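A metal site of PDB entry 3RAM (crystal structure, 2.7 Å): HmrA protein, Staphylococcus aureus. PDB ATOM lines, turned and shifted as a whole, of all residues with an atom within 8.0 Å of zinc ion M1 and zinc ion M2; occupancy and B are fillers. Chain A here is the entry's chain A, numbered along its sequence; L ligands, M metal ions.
The side-chain carboxylate (OD1) of Asp 84 sits at hydrogen-bond distance from a ring nitrogen (ND1) of His 95, 3.0 Å away. The backbone NH (N) of His 341 is in hydrogen-bond range of the backbone carbonyl oxygen (O) of Ala 92. The side-chain carboxylate of Glu 128 sits at hydrogen-bond distance from the side-chain hydroxyl of Thr 315 (2.6 Å). The backbone NH (N) of Glu 129 sits at hydrogen-bond distance from the side-chain carboxylate (OD2) of Asp 84. N of Glu 128 lies within hydrogen-bond range of OD2 of Asp 84 (3.3 Å). A ring nitrogen (NE2) of His 95 lies close to the side-chain carboxylate (OE1) of Glu 82 (3.3 Å).
OE1 of Glu 128 touches zinc ion M1, at 3.2 Å. Of the 23 residues printed, 5 come within 4 Å of zinc ion M1. The nearest printed residue that does not touch zinc ion M1 is Glu 82 (4.1 Å).
Glu 128 touches zinc ion M2. Four residues have an atom within 4 Å of zinc ion M2: Cys 93, Glu 128, Glu 129 and His 341.
Zinc ion M1 is bound by a ring nitrogen (NE2) of His 156, a ring nitrogen (NE2) of His 95 and the side-chain sulfur of Cys 93. Zinc ion M1 has three donor atoms within binding distance. Slightly farther from zinc ion M1 lies an oxygen (O2) of the ligand (2.8 Å).
Zinc ion M2 is bound by OE1 of Glu 129 (2.0 Å), NE2 of His 341 (2.2 Å) and SG of Cys 93 (2.3 Å). Slightly farther from zinc ion M2 lies O2 of the ligand (2.8 Å). Slightly farther from zinc ion M2 lies the side-chain carboxylate (OE2) of Glu 129 (2.8 Å).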
ATOM      1  N   GLU A  82       0.871 -23.039  14.953  1.00  0.00           N
ATOM      2  CA  GLU A  82      -0.159 -23.545  14.040  1.00  0.00           C
ATOM      3  C   GLU A  82       0.477 -24.626  13.140  1.00  0.00           C
ATOM      4  O   GLU A  82       1.679 -24.577  12.844  1.00  0.00           O
ATOM      5  CB  GLU A  82      -0.721 -22.408  13.174  1.00  0.00           C
ATOM      6  CG  GLU A  82      -1.469 -21.290  13.943  1.00  0.00           C
ATOM      7  CD  GLU A  82      -2.023 -20.197  13.029  1.00  0.00           C
ATOM      8  OE1 GLU A  82      -1.755 -20.237  11.808  1.00  0.00           O
ATOM      9  OE2 GLU A  82      -2.732 -19.307  13.537  1.00  0.00           O
ATOM     10  N   ASP A  84      -1.919 -26.965  10.753  1.00  0.00           N
ATOM     11  CA  ASP A  84      -2.936 -27.642   9.910  1.00  0.00           C
ATOM     12  C   ASP A  84      -2.813 -27.281   8.435  1.00  0.00           C
ATOM     13  O   ASP A  84      -2.524 -26.140   8.085  1.00  0.00           O
ATOM     14  CB  ASP A  84      -4.378 -27.355  10.404  1.00  0.00           C
ATOM     15  CG  ASP A  84      -4.755 -25.868  10.385  1.00  0.00           C
ATOM     16  OD1 ASP A  84      -3.936 -25.045  10.865  1.00  0.00           O
ATOM     17  OD2 ASP A  84      -5.873 -25.523   9.937  1.00  0.00           O
ATOM     18  N   ALA A  85      -3.024 -28.276   7.563  1.00  0.00           N
ATOM     19  CA  ALA A  85      -2.978 -28.079   6.105  1.00  0.00           C
ATOM     20  C   ALA A  85      -4.356 -27.720   5.562  1.00  0.00           C
ATOM     21  O   ALA A  85      -5.325 -27.612   6.331  1.00  0.00           O
ATOM     22  CB  ALA A  85      -2.441 -29.333   5.434  1.00  0.00           C
ATOM     23  N   LEU A  86      -4.434 -27.539   4.249  1.00  0.00           N
ATOM     24  CA  LEU A  86      -5.708 -27.318   3.530  1.00  0.00           C
ATOM     25  C   LEU A  86      -6.065 -28.569   2.693  1.00  0.00           C
ATOM     26  O   LEU A  86      -5.164 -29.277   2.237  1.00  0.00           O
ATOM     27  CB  LEU A  86      -5.614 -26.053   2.655  1.00  0.00           C
ATOM     28  CG  LEU A  86      -5.648 -24.699   3.394  1.00  0.00           C
ATOM     29  CD1 LEU A  86      -4.957 -23.598   2.587  1.00  0.00           C
ATOM     30  CD2 LEU A  86      -7.084 -24.301   3.782  1.00  0.00           C
ATOM     31  N   ALA A  92      -0.673 -24.843   1.684  1.00  0.00           N
ATOM     32  CA  ALA A  92      -0.707 -23.659   0.853  1.00  0.00           C
ATOM     33  C   ALA A  92      -0.947 -22.364   1.667  1.00  0.00           C
ATOM     34  O   ALA A  92      -1.150 -21.304   1.067  1.00  0.00           O
ATOM     35  CB  ALA A  92      -1.788 -23.815  -0.239  1.00  0.00           C
ATOM     36  N   CYS A  93      -0.962 -22.459   3.005  1.00  0.00           N
ATOM     37  CA  CYS A  93      -0.906 -21.274   3.885  1.00  0.00           C
ATOM     38  C   CYS A  93       0.386 -21.217   4.712  1.00  0.00           C
ATOM     39  O   CYS A  93       0.570 -20.300   5.518  1.00  0.00           O
ATOM     40  CB  CYS A  93      -2.084 -21.266   4.844  1.00  0.00           C
ATOM     41  SG  CYS A  93      -2.714 -19.611   5.200  1.00  0.00           S
ATOM     42  N   GLY A  94       1.268 -22.197   4.507  1.00  0.00           N
ATOM     43  CA  GLY A  94       2.596 -22.225   5.129  1.00  0.00           C
ATOM     44  C   GLY A  94       2.617 -22.462   6.626  1.00  0.00           C
ATOM     45  O   GLY A  94       3.468 -21.944   7.319  1.00  0.00           O
ATOM     46  N   HIS A  95       1.683 -23.255   7.126  1.00  0.00           N
ATOM     47  CA  HIS A  95       1.558 -23.495   8.566  1.00  0.00           C
ATOM     48  C   HIS A  95       2.653 -24.405   9.152  1.00  0.00           C
ATOM     49  O   HIS A  95       2.853 -24.441  10.375  1.00  0.00           O
ATOM     50  CB  HIS A  95       0.183 -24.055   8.858  1.00  0.00           C
ATOM     51  CG  HIS A  95      -0.886 -23.019   8.830  1.00  0.00           C
ATOM     52  ND1 HIS A  95      -2.148 -23.238   9.344  1.00  0.00           N
ATOM     53  CD2 HIS A  95      -0.878 -21.734   8.397  1.00  0.00           C
ATOM     54  CE1 HIS A  95      -2.876 -22.148   9.191  1.00  0.00           C
ATOM     55  NE2 HIS A  95      -2.128 -21.219   8.631  1.00  0.00           N
ATOM     56  N   ILE A  98       4.897 -21.816  10.670  1.00  0.00           N
ATOM     57  CA  ILE A  98       4.393 -21.090  11.830  1.00  0.00           C
ATOM     58  C   ILE A  98       4.701 -21.880  13.106  1.00  0.00           C
ATOM     59  O   ILE A  98       5.361 -21.364  14.011  1.00  0.00           O
ATOM     60  CB  ILE A  98       2.875 -20.763  11.697  1.00  0.00           C
ATOM     61  CG1 ILE A  98       2.630 -19.950  10.415  1.00  0.00           C
ATOM     62  CG2 ILE A  98       2.381 -20.002  12.920  1.00  0.00           C
ATOM     63  CD1 ILE A  98       1.191 -19.517  10.173  1.00  0.00           C
ATOM     64  N   GLU A 128      -6.829 -23.752  12.547  1.00  0.00           N
ATOM     65  CA  GLU A 128      -7.091 -22.284  12.382  1.00  0.00           C
ATOM     66  C   GLU A 128      -7.790 -21.979  11.079  1.00  0.00           C
ATOM     67  O   GLU A 128      -8.303 -20.886  10.917  1.00  0.00           O
ATOM     68  CB  GLU A 128      -5.835 -21.396  12.503  1.00  0.00           C
ATOM     69  CG  GLU A 128      -5.197 -20.972  11.181  1.00  0.00           C
ATOM     70  CD  GLU A 128      -5.593 -19.597  10.637  1.00  0.00           C
ATOM     71  OE1 GLU A 128      -5.490 -19.395   9.398  1.00  0.00           O
ATOM     72  OE2 GLU A 128      -5.957 -18.710  11.434  1.00  0.00           O
ATOM     73  N   GLU A 129      -7.782 -22.929  10.135  1.00  0.00           N
ATOM     74  CA  GLU A 129      -8.454 -22.739   8.863  1.00  0.00           C
ATOM     75  C   GLU A 129      -9.954 -22.942   9.041  1.00  0.00           C
ATOM     76  O   GLU A 129     -10.722 -22.597   8.152  1.00  0.00           O
ATOM     77  CB  GLU A 129      -7.886 -23.689   7.809  1.00  0.00           C
ATOM     78  CG  GLU A 129      -6.412 -23.409   7.437  1.00  0.00           C
ATOM     79  CD  GLU A 129      -6.215 -22.094   6.688  1.00  0.00           C
ATOM     80  OE1 GLU A 129      -5.056 -21.736   6.402  1.00  0.00           O
ATOM     81  OE2 GLU A 129      -7.218 -21.423   6.390  1.00  0.00           O
ATOM     82  N   GLY A 130     -10.366 -23.459  10.184  1.00  0.00           N
ATOM     83  CA  GLY A 130     -11.788 -23.545  10.531  1.00  0.00           C
ATOM     84  C   GLY A 130     -12.352 -24.900  10.203  1.00  0.00           C
ATOM     85  O   GLY A 130     -11.599 -25.799   9.840  1.00  0.00           O
ATOM     86  N   MET A 154       3.622 -14.583  17.413  1.00  0.00           N
ATOM     87  CA  MET A 154       3.381 -15.423  16.240  1.00  0.00           C
ATOM     88  C   MET A 154       3.909 -14.718  14.985  1.00  0.00           C
ATOM     89  O   MET A 154       4.006 -13.499  14.967  1.00  0.00           O
ATOM     90  CB  MET A 154       1.890 -15.588  16.099  1.00  0.00           C
ATOM     91  CG  MET A 154       1.461 -16.566  15.050  1.00  0.00           C
ATOM     92  SD  MET A 154      -0.414 -16.240  14.644  1.00  0.00           S
ATOM     93  CE  MET A 154      -0.445 -17.162  12.887  1.00  0.00           C
ATOM     94  N   ILE A 155       4.260 -15.486  13.954  1.00  0.00           N
ATOM     95  CA  ILE A 155       4.565 -14.912  12.639  1.00  0.00           C
ATOM     96  C   ILE A 155       3.844 -15.752  11.576  1.00  0.00           C
ATOM     97  O   ILE A 155       3.606 -16.949  11.785  1.00  0.00           O
ATOM     98  CB  ILE A 155       6.087 -14.812  12.336  1.00  0.00           C
ATOM     99  CG1 ILE A 155       6.747 -16.204  12.277  1.00  0.00           C
ATOM    100  CG2 ILE A 155       6.784 -13.907  13.371  1.00  0.00           C
ATOM    101  CD1 ILE A 155       6.625 -16.936  10.923  1.00  0.00           C
ATOM    102  N   HIS A 156       3.446 -15.115  10.469  1.00  0.00           N
ATOM    103  CA  HIS A 156       2.720 -15.776   9.398  1.00  0.00           C
ATOM    104  C   HIS A 156       3.389 -15.561   8.029  1.00  0.00           C
ATOM    105  O   HIS A 156       3.467 -14.424   7.557  1.00  0.00           O
ATOM    106  CB  HIS A 156       1.245 -15.317   9.343  1.00  0.00           C
ATOM    107  CG  HIS A 156       0.354 -16.273   8.603  1.00  0.00           C
ATOM    108  ND1 HIS A 156       0.524 -16.589   7.275  1.00  0.00           N
ATOM    109  CD2 HIS A 156      -0.709 -17.006   9.028  1.00  0.00           C
ATOM    110  CE1 HIS A 156      -0.386 -17.460   6.908  1.00  0.00           C
ATOM    111  NE2 HIS A 156      -1.146 -17.735   7.948  1.00  0.00           N
ATOM    112  N   PRO A 157       3.837 -16.637   7.362  1.00  0.00           N
ATOM    113  CA  PRO A 157       4.491 -16.427   6.082  1.00  0.00           C
ATOM    114  C   PRO A 157       3.586 -15.659   5.115  1.00  0.00           C
ATOM    115  O   PRO A 157       2.384 -15.883   5.119  1.00  0.00           O
ATOM    116  CB  PRO A 157       4.755 -17.854   5.567  1.00  0.00           C
ATOM    117  CG  PRO A 157       3.993 -18.764   6.432  1.00  0.00           C
ATOM    118  CD  PRO A 157       3.796 -18.070   7.730  1.00  0.00           C
ATOM    119  N   SER A 314      -8.687 -13.068   8.775  1.00  0.00           N
ATOM    120  CA  SER A 314      -9.818 -13.736   9.377  1.00  0.00           C
ATOM    121  C   SER A 314      -9.315 -14.962  10.129  1.00  0.00           C
ATOM    122  O   SER A 314      -9.381 -16.084   9.605  1.00  0.00           O
ATOM    123  CB  SER A 314     -10.822 -14.119   8.281  1.00  0.00           C
ATOM    124  OG  SER A 314     -12.106 -14.292   8.840  1.00  0.00           O
ATOM    125  N   THR A 315      -8.821 -14.732  11.343  1.00  0.00           N
ATOM    126  CA  THR A 315      -8.065 -15.753  12.087  1.00  0.00           C
ATOM    127  C   THR A 315      -8.485 -15.768  13.550  1.00  0.00           C
ATOM    128  O   THR A 315      -8.836 -14.730  14.109  1.00  0.00           O
ATOM    129  CB  THR A 315      -6.541 -15.473  11.984  1.00  0.00           C
ATOM    130  OG1 THR A 315      -5.818 -16.477  12.689  1.00  0.00           O
ATOM    131  CG2 THR A 315      -6.185 -14.077  12.549  1.00  0.00           C
ATOM    132  N   HIS A 328      -0.118 -10.670  14.835  1.00  0.00           N
ATOM    133  CA  HIS A 328      -0.320 -11.583  13.715  1.00  0.00           C
ATOM    134  C   HIS A 328       0.293 -10.906  12.492  1.00  0.00           C
ATOM    135  O   HIS A 328      -0.425 -10.395  11.631  1.00  0.00           O
ATOM    136  CB  HIS A 328      -1.803 -11.870  13.529  1.00  0.00           C
ATOM    137  CG  HIS A 328      -2.118 -12.767  12.371  1.00  0.00           C
ATOM    138  ND1 HIS A 328      -2.707 -12.299  11.213  1.00  0.00           N
ATOM    139  CD2 HIS A 328      -1.966 -14.102  12.196  1.00  0.00           C
ATOM    140  CE1 HIS A 328      -2.892 -13.316  10.379  1.00  0.00           C
ATOM    141  NE2 HIS A 328      -2.444 -14.419  10.948  1.00  0.00           N
ATOM    142  N   HIS A 330       3.353 -10.716   9.204  1.00  0.00           N
ATOM    143  CA  HIS A 330       3.776 -11.590   8.142  1.00  0.00           C
ATOM    144  C   HIS A 330       5.286 -11.467   7.867  1.00  0.00           C
ATOM    145  O   HIS A 330       5.879 -10.408   8.068  1.00  0.00           O
ATOM    146  CB  HIS A 330       2.963 -11.245   6.903  1.00  0.00           C
ATOM    147  CG  HIS A 330       1.570 -11.807   6.913  1.00  0.00           C
ATOM    148  ND1 HIS A 330       0.551 -11.255   7.676  1.00  0.00           N
ATOM    149  CD2 HIS A 330       1.005 -12.825   6.223  1.00  0.00           C
ATOM    150  CE1 HIS A 330      -0.562 -11.929   7.459  1.00  0.00           C
ATOM    151  NE2 HIS A 330      -0.315 -12.878   6.583  1.00  0.00           N
ATOM    152  N   GLY A 340      -1.893 -16.312  -0.830  1.00  0.00           N
ATOM    153  CA  GLY A 340      -2.140 -17.428   0.096  1.00  0.00           C
ATOM    154  C   GLY A 340      -3.128 -18.437  -0.471  1.00  0.00           C
ATOM    155  O   GLY A 340      -3.945 -18.087  -1.340  1.00  0.00           O
ATOM    156  N   HIS A 341      -3.040 -19.666   0.036  1.00  0.00           N
ATOM    157  CA  HIS A 341      -3.884 -20.798  -0.388  1.00  0.00           C
ATOM    158  C   HIS A 341      -3.792 -21.118  -1.910  1.00  0.00           C
ATOM    159  O   HIS A 341      -4.783 -21.474  -2.541  1.00  0.00           O
ATOM    160  CB  HIS A 341      -5.356 -20.554  -0.024  1.00  0.00           C
ATOM    161  CG  HIS A 341      -5.632 -20.503   1.442  1.00  0.00           C
ATOM    162  ND1 HIS A 341      -6.869 -20.830   1.965  1.00  0.00           N
ATOM    163  CD2 HIS A 341      -4.855 -20.159   2.494  1.00  0.00           C
ATOM    164  CE1 HIS A 341      -6.836 -20.681   3.276  1.00  0.00           C
ATOM    165  NE2 HIS A 341      -5.633 -20.283   3.627  1.00  0.00           N
ATOM    166  N   PHE A 345       2.127 -21.004  -3.244  1.00  0.00           N
ATOM    167  CA  PHE A 345       2.404 -20.661  -1.849  1.00  0.00           C
ATOM    168  C   PHE A 345       2.946 -21.869  -1.100  1.00  0.00           C
ATOM    169  O   PHE A 345       3.921 -21.751  -0.362  1.00  0.00           O
ATOM    170  CB  PHE A 345       1.151 -20.112  -1.174  1.00  0.00           C
ATOM    171  CG  PHE A 345       1.432 -19.254   0.049  1.00  0.00           C
ATOM    172  CD1 PHE A 345       1.501 -17.870  -0.064  1.00  0.00           C
ATOM    173  CD2 PHE A 345       1.611 -19.828   1.297  1.00  0.00           C
ATOM    174  CE1 PHE A 345       1.747 -17.082   1.040  1.00  0.00           C
ATOM    175  CE2 PHE A 345       1.866 -19.047   2.392  1.00  0.00           C
ATOM    176  CZ  PHE A 345       1.922 -17.677   2.267  1.00  0.00           C
HETATM  177  C1  LIG L   1      -7.254 -17.609   6.921  1.00  0.00           C
HETATM  178  O1  LIG L   1      -8.279 -18.034   7.798  1.00  0.00           O
HETATM  179  C2  LIG L   1      -6.092 -16.974   7.697  1.00  0.00           C
HETATM  180  O2  LIG L   1      -4.960 -17.811   7.568  1.00  0.00           O
HETATM  181  C3  LIG L   1      -5.855 -15.532   7.190  1.00  0.00           C
HETATM  182  O3  LIG L   1      -4.829 -14.794   7.868  1.00  0.00           O
HETATM  183 ZN    ZN M   1      -2.645 -19.261   7.913  1.00  0.00          ZN
HETATM  184 ZN    ZN M   2      -5.011 -19.841   5.638  1.00  0.00          ZN
